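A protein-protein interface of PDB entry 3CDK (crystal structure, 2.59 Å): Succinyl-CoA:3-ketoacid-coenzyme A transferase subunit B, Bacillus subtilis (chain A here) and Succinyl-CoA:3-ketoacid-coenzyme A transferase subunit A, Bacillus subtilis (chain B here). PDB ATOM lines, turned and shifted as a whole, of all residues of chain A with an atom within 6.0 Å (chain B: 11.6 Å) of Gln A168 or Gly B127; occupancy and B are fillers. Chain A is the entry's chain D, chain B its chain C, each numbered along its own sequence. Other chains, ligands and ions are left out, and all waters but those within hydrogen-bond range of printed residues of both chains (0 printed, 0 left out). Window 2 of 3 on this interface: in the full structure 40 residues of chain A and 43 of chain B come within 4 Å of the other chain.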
ATOM      1  N   GLN A 113      14.951  -7.137   1.751  1.00  0.00           N
ATOM      2  CA  GLN A 113      14.406  -5.773   1.674  1.00  0.00           C
ATOM      3  C   GLN A 113      15.187  -4.945   0.654  1.00  0.00           C
ATOM      4  O   GLN A 113      14.970  -3.730   0.499  1.00  0.00           O
ATOM      5  CB  GLN A 113      14.451  -5.062   3.028  1.00  0.00           C
ATOM      6  CG  GLN A 113      14.637  -5.940   4.257  1.00  0.00           C
ATOM      7  CD  GLN A 113      15.255  -5.173   5.433  1.00  0.00           C
ATOM      8  OE1 GLN A 113      15.850  -4.082   5.268  1.00  0.00           O
ATOM      9  NE2 GLN A 113      15.121  -5.746   6.631  1.00  0.00           N
ATOM     10  N   GLY A 114      16.105  -5.613  -0.036  1.00  0.00           N
ATOM     11  CA  GLY A 114      16.984  -4.943  -0.966  1.00  0.00           C
ATOM     12  C   GLY A 114      18.040  -4.120  -0.249  1.00  0.00           C
ATOM     13  O   GLY A 114      18.272  -2.969  -0.602  1.00  0.00           O
ATOM     14  N   ASP A 115      18.667  -4.688   0.774  1.00  0.00           N
ATOM     15  CA  ASP A 115      19.900  -4.104   1.265  1.00  0.00           C
ATOM     16  C   ASP A 115      21.017  -4.627   0.379  1.00  0.00           C
ATOM     17  O   ASP A 115      20.955  -5.762  -0.106  1.00  0.00           O
ATOM     18  CB  ASP A 115      20.170  -4.473   2.720  1.00  0.00           C
ATOM     19  CG  ASP A 115      19.009  -4.142   3.638  1.00  0.00           C
ATOM     20  OD1 ASP A 115      18.123  -3.340   3.254  1.00  0.00           O
ATOM     21  OD2 ASP A 115      18.977  -4.704   4.757  1.00  0.00           O
ATOM     22  N   LEU A 116      22.029  -3.801   0.154  1.00  0.00           N
ATOM     23  CA  LEU A 116      23.188  -4.238  -0.605  1.00  0.00           C
ATOM     24  C   LEU A 116      24.454  -4.207   0.237  1.00  0.00           C
ATOM     25  O   LEU A 116      24.675  -3.281   1.015  1.00  0.00           O
ATOM     26  CB  LEU A 116      23.363  -3.400  -1.875  1.00  0.00           C
ATOM     27  CG  LEU A 116      24.595  -3.700  -2.731  1.00  0.00           C
ATOM     28  CD1 LEU A 116      24.338  -4.877  -3.665  1.00  0.00           C
ATOM     29  CD2 LEU A 116      24.981  -2.455  -3.492  1.00  0.00           C
ATOM     30  N   VAL A 136      24.254   4.727  -4.216  1.00  0.00           N
ATOM     31  CA  VAL A 136      23.123   3.980  -3.689  1.00  0.00           C
ATOM     32  C   VAL A 136      22.057   4.854  -2.993  1.00  0.00           C
ATOM     33  O   VAL A 136      20.885   4.506  -2.974  1.00  0.00           O
ATOM     34  CB  VAL A 136      23.679   2.810  -2.817  1.00  0.00           C
ATOM     35  CG1 VAL A 136      23.191   2.847  -1.386  1.00  0.00           C
ATOM     36  CG2 VAL A 136      23.429   1.454  -3.501  1.00  0.00           C
ATOM     37  N   ASN A 137      22.471   6.000  -2.445  1.00  0.00           N
ATOM     38  CA  ASN A 137      21.536   6.910  -1.783  1.00  0.00           C
ATOM     39  C   ASN A 137      21.091   8.113  -2.645  1.00  0.00           C
ATOM     40  O   ASN A 137      20.134   8.787  -2.292  1.00  0.00           O
ATOM     41  CB  ASN A 137      22.073   7.376  -0.412  1.00  0.00           C
ATOM     42  CG  ASN A 137      22.362   6.215   0.549  1.00  0.00           C
ATOM     43  OD1 ASN A 137      21.489   5.392   0.856  1.00  0.00           O
ATOM     44  ND2 ASN A 137      23.602   6.149   1.032  1.00  0.00           N
ATOM     45  N   LEU A 165      26.903  -3.613   5.194  1.00  0.00           N
ATOM     46  CA  LEU A 165      26.008  -3.005   4.202  1.00  0.00           C
ATOM     47  C   LEU A 165      26.621  -1.817   3.507  1.00  0.00           C
ATOM     48  O   LEU A 165      27.237  -0.987   4.149  1.00  0.00           O
ATOM     49  CB  LEU A 165      24.682  -2.572   4.847  1.00  0.00           C
ATOM     50  CG  LEU A 165      23.674  -3.672   5.203  1.00  0.00           C
ATOM     51  CD1 LEU A 165      22.336  -3.113   5.694  1.00  0.00           C
ATOM     52  CD2 LEU A 165      23.451  -4.609   4.003  1.00  0.00           C
ATOM     53  N   THR A 166      26.451  -1.760   2.188  1.00  0.00           N
ATOM     54  CA  THR A 166      26.786  -0.603   1.366  1.00  0.00           C
ATOM     55  C   THR A 166      25.639   0.381   1.522  1.00  0.00           C
ATOM     56  O   THR A 166      25.828   1.612   1.598  1.00  0.00           O
ATOM     57  CB  THR A 166      26.865  -1.006  -0.126  1.00  0.00           C
ATOM     58  OG1 THR A 166      27.982  -1.873  -0.317  1.00  0.00           O
ATOM     59  CG2 THR A 166      27.030   0.200  -1.024  1.00  0.00           C
ATOM     60  N   GLY A 167      24.448  -0.214   1.572  1.00  0.00           N
ATOM     61  CA  GLY A 167      23.191   0.506   1.592  1.00  0.00           C
ATOM     62  C   GLY A 167      22.058  -0.370   2.077  1.00  0.00           C
ATOM     63  O   GLY A 167      22.065  -1.599   1.913  1.00  0.00           O
ATOM     64  N   GLN A 168      21.066   0.286   2.659  1.00  0.00           N
ATOM     65  CA  GLN A 168      19.982  -0.397   3.325  1.00  0.00           C
ATOM     66  C   GLN A 168      18.660   0.014   2.685  1.00  0.00           C
ATOM     67  O   GLN A 168      18.261   1.177   2.748  1.00  0.00           O
ATOM     68  CB  GLN A 168      20.052  -0.030   4.799  1.00  0.00           C
ATOM     69  CG  GLN A 168      18.903  -0.429   5.659  1.00  0.00           C
ATOM     70  CD  GLN A 168      19.096   0.107   7.052  1.00  0.00           C
ATOM     71  OE1 GLN A 168      19.036   1.318   7.274  1.00  0.00           O
ATOM     72  NE2 GLN A 168      19.373  -0.781   7.996  1.00  0.00           N
ATOM     73  N   LYS A 169      18.009  -0.958   2.055  1.00  0.00           N
ATOM     74  CA  LYS A 169      16.744  -0.770   1.335  1.00  0.00           C
ATOM     75  C   LYS A 169      16.949   0.163   0.153  1.00  0.00           C
ATOM     76  O   LYS A 169      16.166   1.089  -0.060  1.00  0.00           O
ATOM     77  CB  LYS A 169      15.626  -0.234   2.245  1.00  0.00           C
ATOM     78  CG  LYS A 169      15.373  -1.019   3.542  1.00  0.00           C
ATOM     79  CD  LYS A 169      13.873  -1.143   3.866  1.00  0.00           C
ATOM     80  CE  LYS A 169      13.103   0.182   3.768  1.00  0.00           C
ATOM     81  NZ  LYS A 169      11.617  -0.061   3.765  1.00  0.00           N
ATOM     82  N   VAL A 170      17.991  -0.086  -0.626  1.00  0.00           N
ATOM     83  CA  VAL A 170      18.364   0.870  -1.651  1.00  0.00           C
ATOM     84  C   VAL A 170      18.158   0.402  -3.083  1.00  0.00           C
ATOM     85  O   VAL A 170      17.976   1.235  -3.978  1.00  0.00           O
ATOM     86  CB  VAL A 170      19.800   1.350  -1.478  1.00  0.00           C
ATOM     87  CG1 VAL A 170      19.872   2.325  -0.311  1.00  0.00           C
ATOM     88  CG2 VAL A 170      20.723   0.155  -1.291  1.00  0.00           C
ATOM     89  N   PRO B 102      33.060   7.623   2.717  1.00  0.00           N
ATOM     90  CA  PRO B 102      32.519   7.541   1.358  1.00  0.00           C
ATOM     91  C   PRO B 102      33.068   8.672   0.496  1.00  0.00           C
ATOM     92  O   PRO B 102      33.369   9.744   1.002  1.00  0.00           O
ATOM     93  CB  PRO B 102      31.019   7.671   1.573  1.00  0.00           C
ATOM     94  CG  PRO B 102      30.792   7.149   3.030  1.00  0.00           C
ATOM     95  CD  PRO B 102      32.002   7.651   3.753  1.00  0.00           C
ATOM     96  N   THR B 122      24.201  14.809   5.200  1.00  0.00           N
ATOM     97  CA  THR B 122      24.121  14.000   3.973  1.00  0.00           C
ATOM     98  C   THR B 122      23.427  12.684   4.288  1.00  0.00           C
ATOM     99  O   THR B 122      23.467  12.260   5.448  1.00  0.00           O
ATOM    100  CB  THR B 122      25.540  13.745   3.354  1.00  0.00           C
ATOM    101  OG1 THR B 122      25.418  12.774   2.334  1.00  0.00           O
ATOM    102  CG2 THR B 122      26.536  13.215   4.392  1.00  0.00           C
ATOM    103  N   ALA B 123      22.820  12.042   3.282  1.00  0.00           N
ATOM    104  CA  ALA B 123      22.205  10.702   3.437  1.00  0.00           C
ATOM    105  C   ALA B 123      23.215   9.571   3.228  1.00  0.00           C
ATOM    106  O   ALA B 123      22.959   8.416   3.577  1.00  0.00           O
ATOM    107  CB  ALA B 123      21.095  10.538   2.463  1.00  0.00           C
ATOM    108  N   THR B 124      24.346   9.872   2.604  1.00  0.00           N
ATOM    109  CA  THR B 124      25.346   8.839   2.321  1.00  0.00           C
ATOM    110  C   THR B 124      25.802   8.034   3.544  1.00  0.00           C
ATOM    111  O   THR B 124      26.398   8.573   4.449  1.00  0.00           O
ATOM    112  CB  THR B 124      26.535   9.453   1.560  1.00  0.00           C
ATOM    113  OG1 THR B 124      26.021  10.017   0.344  1.00  0.00           O
ATOM    114  CG2 THR B 124      27.555   8.434   1.242  1.00  0.00           C
ATOM    115  N   GLY B 125      25.499   6.747   3.567  1.00  0.00           N
ATOM    116  CA  GLY B 125      25.964   5.870   4.639  1.00  0.00           C
ATOM    117  C   GLY B 125      25.042   5.658   5.850  1.00  0.00           C
ATOM    118  O   GLY B 125      25.425   4.948   6.800  1.00  0.00           O
ATOM    119  N   VAL B 126      23.847   6.260   5.854  1.00  0.00           N
ATOM    120  CA  VAL B 126      22.914   5.959   6.938  1.00  0.00           C
ATOM    121  C   VAL B 126      22.490   4.498   6.852  1.00  0.00           C
ATOM    122  O   VAL B 126      22.453   3.913   5.760  1.00  0.00           O
ATOM    123  CB  VAL B 126      21.701   6.956   7.054  1.00  0.00           C
ATOM    124  CG1 VAL B 126      21.998   8.246   6.310  1.00  0.00           C
ATOM    125  CG2 VAL B 126      20.382   6.319   6.644  1.00  0.00           C
ATOM    126  N   GLY B 127      22.244   3.889   8.002  1.00  0.00           N
ATOM    127  CA  GLY B 127      21.869   2.476   8.022  1.00  0.00           C
ATOM    128  C   GLY B 127      23.074   1.563   7.882  1.00  0.00           C
ATOM    129  O   GLY B 127      22.925   0.332   7.911  1.00  0.00           O
ATOM    130  N   THR B 128      24.259   2.163   7.741  1.00  0.00           N
ATOM    131  CA  THR B 128      25.515   1.413   7.676  1.00  0.00           C
ATOM    132  C   THR B 128      26.442   1.742   8.853  1.00  0.00           C
ATOM    133  O   THR B 128      26.209   2.713   9.590  1.00  0.00           O
ATOM    134  CB  THR B 128      26.282   1.618   6.322  1.00  0.00           C
ATOM    135  OG1 THR B 128      26.793   2.954   6.231  1.00  0.00           O
ATOM    136  CG2 THR B 128      25.380   1.358   5.150  1.00  0.00           C
ATOM    137  N   SER B 129      27.492   0.928   9.009  1.00  0.00           N
ATOM    138  CA  SER B 129      28.488   1.089  10.063  1.00  0.00           C
ATOM    139  C   SER B 129      29.244   2.421   9.971  1.00  0.00           C
ATOM    140  O   SER B 129      29.836   2.869  10.957  1.00  0.00           O
ATOM    141  CB  SER B 129      29.487  -0.067  10.013  1.00  0.00           C
ATOM    142  OG  SER B 129      30.130  -0.125   8.749  1.00  0.00           O
ATOM    143  N   ILE B 130      29.219   3.051   8.798  1.00  0.00           N
ATOM    144  CA  ILE B 130      29.868   4.359   8.587  1.00  0.00           C
ATOM    145  C   ILE B 130      29.245   5.469   9.427  1.00  0.00           C
ATOM    146  O   ILE B 130      29.929   6.383   9.881  1.00  0.00           O
ATOM    147  CB  ILE B 130      29.931   4.724   7.062  1.00  0.00           C
ATOM    148  CG1 ILE B 130      31.374   4.671   6.547  1.00  0.00           C
ATOM    149  CG2 ILE B 130      29.352   6.129   6.754  1.00  0.00           C
ATOM    150  CD1 ILE B 130      32.174   3.453   6.942  1.00  0.00           C
ATOM    151  N   ALA B 131      27.946   5.367   9.668  1.00  0.00           N
ATOM    152  CA  ALA B 131      27.253   6.399  10.407  1.00  0.00           C
ATOM    153  C   ALA B 131      27.257   6.161  11.918  1.00  0.00           C
ATOM    154  O   ALA B 131      26.785   7.013  12.657  1.00  0.00           O
ATOM    155  CB  ALA B 131      25.834   6.547   9.894  1.00  0.00           C
ATOM    156  N   GLU B 132      27.785   5.037  12.393  1.00  0.00           N
ATOM    157  CA  GLU B 132      27.839   4.835  13.851  1.00  0.00           C
ATOM    158  C   GLU B 132      28.736   5.867  14.554  1.00  0.00           C
ATOM    159  O   GLU B 132      29.808   6.201  14.042  1.00  0.00           O
ATOM    160  CB  GLU B 132      28.162   3.380  14.231  1.00  0.00           C
ATOM    161  CG  GLU B 132      26.894   2.571  14.586  1.00  0.00           C
ATOM    162  CD  GLU B 132      27.117   1.065  14.636  1.00  0.00           C
ATOM    163  OE1 GLU B 132      28.055   0.563  13.977  1.00  0.00           O
ATOM    164  OE2 GLU B 132      26.334   0.366  15.326  1.00  0.00           O
ATOM    165  N   GLY B 133      28.242   6.412  15.677  1.00  0.00           N
ATOM    166  CA  GLY B 133      28.935   7.451  16.459  1.00  0.00           C
ATOM    167  C   GLY B 133      28.787   8.929  16.050  1.00  0.00           C
ATOM    168  O   GLY B 133      29.453   9.816  16.640  1.00  0.00           O
ATOM    169  N   LYS B 134      27.928   9.211  15.062  1.00  0.00           N
ATOM    170  CA  LYS B 134      27.728  10.583  14.580  1.00  0.00           C
ATOM    171  C   LYS B 134      26.298  11.093  14.758  1.00  0.00           C
ATOM    172  O   LYS B 134      25.363  10.311  14.746  1.00  0.00           O
ATOM    173  CB  LYS B 134      28.074  10.684  13.110  1.00  0.00           C
ATOM    174  CG  LYS B 134      29.457  10.201  12.731  1.00  0.00           C
ATOM    175  CD  LYS B 134      29.526  10.050  11.215  1.00  0.00           C
ATOM    176  CE  LYS B 134      30.933   9.748  10.739  1.00  0.00           C
ATOM    177  NZ  LYS B 134      30.824   9.250   9.359  1.00  0.00           N
ATOM    178  N   GLU B 135      26.133  12.412  14.886  1.00  0.00           N
ATOM    179  CA  GLU B 135      24.816  13.006  15.020  1.00  0.00           C
ATOM    180  C   GLU B 135      23.911  12.655  13.830  1.00  0.00           C
ATOM    181  O   GLU B 135      24.323  12.705  12.669  1.00  0.00           O
ATOM    182  CB  GLU B 135      24.917  14.520  15.175  1.00  0.00           C
ATOM    183  CG  GLU B 135      25.476  15.000  16.482  1.00  0.00           C
ATOM    184  CD  GLU B 135      26.983  15.196  16.434  1.00  0.00           C
ATOM    185  OE1 GLU B 135      27.655  14.560  15.571  1.00  0.00           O
ATOM    186  OE2 GLU B 135      27.511  15.988  17.254  1.00  0.00           O
ATOM    187  N   HIS B 136      22.671  12.311  14.144  1.00  0.00           N
ATOM    188  CA  HIS B 136      21.638  12.040  13.155  1.00  0.00           C
ATOM    189  C   HIS B 136      20.571  13.118  13.258  1.00  0.00           C
ATOM    190  O   HIS B 136      20.183  13.543  14.346  1.00  0.00           O
ATOM    191  CB  HIS B 136      21.019  10.673  13.425  1.00  0.00           C
ATOM    192  CG  HIS B 136      21.872   9.531  12.977  1.00  0.00           C
ATOM    193  ND1 HIS B 136      23.203   9.411  13.322  1.00  0.00           N
ATOM    194  CD2 HIS B 136      21.581   8.444  12.224  1.00  0.00           C
ATOM    195  CE1 HIS B 136      23.699   8.311  12.788  1.00  0.00           C
ATOM    196  NE2 HIS B 136      22.736   7.705  12.116  1.00  0.00           N
ATOM    197  N   LYS B 137      20.093  13.564  12.116  1.00  0.00           N
ATOM    198  CA  LYS B 137      19.062  14.594  12.088  1.00  0.00           C
ATOM    199  C   LYS B 137      18.102  14.309  10.938  1.00  0.00           C
ATOM    200  O   LYS B 137      18.510  13.874   9.848  1.00  0.00           O
ATOM    201  CB  LYS B 137      19.698  15.966  11.940  1.00  0.00           C
ATOM    202  CG  LYS B 137      18.765  17.139  12.191  1.00  0.00           C
ATOM    203  CD  LYS B 137      19.558  18.440  12.317  1.00  0.00           C
ATOM    204  CE  LYS B 137      18.625  19.638  12.337  1.00  0.00           C
ATOM    205  NZ  LYS B 137      17.717  19.689  13.559  1.00  0.00           N
ATOM    206  N   ARG B 142      13.268  12.367   6.334  1.00  0.00           N
ATOM    207  CA  ARG B 142      14.404  11.464   6.060  1.00  0.00           C
ATOM    208  C   ARG B 142      15.584  11.777   6.964  1.00  0.00           C
ATOM    209  O   ARG B 142      15.820  12.941   7.336  1.00  0.00           O
ATOM    210  CB  ARG B 142      14.884  11.593   4.596  1.00  0.00           C
ATOM    211  CG  ARG B 142      13.926  11.006   3.552  1.00  0.00           C
ATOM    212  CD  ARG B 142      13.944  11.821   2.225  1.00  0.00           C
ATOM    213  NE  ARG B 142      12.590  12.022   1.684  1.00  0.00           N
ATOM    214  CZ  ARG B 142      11.803  11.057   1.169  1.00  0.00           C
ATOM    215  NH1 ARG B 142      12.226   9.779   1.102  1.00  0.00           N
ATOM    216  NH2 ARG B 142      10.576  11.371   0.722  1.00  0.00           N
ATOM    217  N   THR B 143      16.348  10.729   7.263  1.00  0.00           N
ATOM    218  CA  THR B 143      17.468  10.780   8.207  1.00  0.00           C
ATOM    219  C   THR B 143      18.815  11.049   7.525  1.00  0.00           C
ATOM    220  O   THR B 143      19.141  10.443   6.510  1.00  0.00           O
ATOM    221  CB  THR B 143      17.511   9.491   9.066  1.00  0.00           C
ATOM    222  OG1 THR B 143      16.229   9.309   9.665  1.00  0.00           O
ATOM    223  CG2 THR B 143      18.544   9.588  10.188  1.00  0.00           C
ATOM    224  N   TYR B 144      19.569  11.986   8.098  1.00  0.00           N
ATOM    225  CA  TYR B 144      20.896  12.390   7.608  1.00  0.00           C
ATOM    226  C   TYR B 144      21.968  12.289   8.722  1.00  0.00           C
ATOM    227  O   TYR B 144      21.634  12.272   9.938  1.00  0.00           O
ATOM    228  CB  TYR B 144      20.831  13.811   7.033  1.00  0.00           C
ATOM    229  CG  TYR B 144      19.860  13.940   5.856  1.00  0.00           C
ATOM    230  CD1 TYR B 144      18.485  14.137   6.071  1.00  0.00           C
ATOM    231  CD2 TYR B 144      20.306  13.819   4.524  1.00  0.00           C
ATOM    232  CE1 TYR B 144      17.591  14.217   4.997  1.00  0.00           C
ATOM    233  CE2 TYR B 144      19.410  13.914   3.446  1.00  0.00           C
ATOM    234  CZ  TYR B 144      18.070  14.122   3.707  1.00  0.00           C
ATOM    235  OH  TYR B 144      17.190  14.230   2.686  1.00  0.00           O
ATOM    236  N   VAL B 145      23.231  12.150   8.316  1.00  0.00           N
ATOM    237  CA  VAL B 145      24.345  12.159   9.258  1.00  0.00           C
ATOM    238  C   VAL B 145      25.103  13.466   9.169  1.00  0.00           C
ATOM    239  O   VAL B 145      25.348  13.952   8.082  1.00  0.00           O
ATOM    240  CB  VAL B 145      25.429  11.105   8.931  1.00  0.00           C
ATOM    241  CG1 VAL B 145      26.057  10.604  10.220  1.00  0.00           C
ATOM    242  CG2 VAL B 145      24.890   9.970   8.094  1.00  0.00           C
ATOM    243  N   LEU B 146      25.518  13.997  10.314  1.00  0.00           N
ATOM    244  CA  LEU B 146      26.427  15.143  10.321  1.00  0.00           C
ATOM    245  C   LEU B 146      27.816  14.704   9.910  1.00  0.00           C
ATOM    246  O   LEU B 146      28.400  13.809  10.553  1.00  0.00           O
ATOM    247  CB  LEU B 146      26.476  15.738  11.720  1.00  0.00           C
ATOM    248  CG  LEU B 146      27.394  16.915  12.012  1.00  0.00           C
ATOM    249  CD1 LEU B 146      27.072  18.024  11.070  1.00  0.00           C
ATOM    250  CD2 LEU B 146      27.211  17.357  13.455  1.00  0.00           C
ATOM    251  N   GLU B 147      28.359  15.314   8.857  1.00  0.00           N
ATOM    252  CA  GLU B 147      29.773  15.144   8.546  1.00  0.00           C
ATOM    253  C   GLU B 147      30.580  16.445   8.763  1.00  0.00           C
ATOM    254  O   GLU B 147      30.110  17.553   8.462  1.00  0.00           O
ATOM    255  CB  GLU B 147      29.927  14.576   7.141  1.00  0.00           C
ATOM    256  CG  GLU B 147      29.294  13.177   6.957  1.00  0.00           C
ATOM    257  CD  GLU B 147      30.138  11.958   7.541  1.00  0.00           C
ATOM    258  OE1 GLU B 147      31.301  12.096   7.993  1.00  0.00           O
ATOM    259  OE2 GLU B 147      29.630  10.816   7.518  1.00  0.00           O
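Printed residues of chain A that touch a printed residue of chain B: Asn A137, Leu A165, Thr A166 and Gln A168. Of the 23 printed residues of chain B, 5 touch a printed residue of chain A. Along chain B the printed residues that touch a printed residue of chain A span positions 123 to 128.
ND2 of Asn A137 touches CA of Thr B124, at 3.5 Å. Leu A165 touches Thr B128. CG2 of Thr B128 touches O of Thr A166 (3.6 Å). Gln A168 touches Gly B127 (OE1 to CA, 3.2 Å).
Gln A168 touches one residue of chain B. No residue of chain B comes within 4 Å of Gly A114. No residue of chain B comes within 4 Å of Asp A115. Leu A165 touches just one residue of chain B: Thr B128 (3.2 Å). No residue of chain B comes within 4 Å of Lys A169. Val A170 touches none of the printed residues of chain B. Of the printed residues of chain A, Gly B125 touches Asn A137. Printed residues of chain A within 4 Å of Thr B124: Asn A137 (3.5 Å). Of the printed residues of chain A, Thr B128 touches Leu A165 and Thr A166. Of the printed residues of chain A, Ala B123 touches Asn A137. Pro B102 touches none of the printed residues of chain A. Gly B133 touches none of the printed residues of chain A. The nearest residue of chain A that does not touch Gly B127 is Leu A165 (4.1 Å).
The side-chain hydroxyl of Thr B122 lies within hydrogen-bond range of the backbone NH of Thr B124 (3.1 Å). The side-chain hydroxyl (OG1) of Thr B128 sits at hydrogen-bond distance from the backbone carbonyl oxygen (O) of Gly B125, 2.5 Å away. O of Leu A116 sits at hydrogen-bond distance from N of Thr A166 (2.6 Å).
The side-chain amide nitrogen (ND2) of Asn A137 is in hydrogen-bond range of the backbone carbonyl oxygen (O) of Ala B123, 3.5 Å away. The side-chain amide nitrogen (ND2) of Asn A137 lies close to the backbone NH (N) of Gly B125 (3.2 Å).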
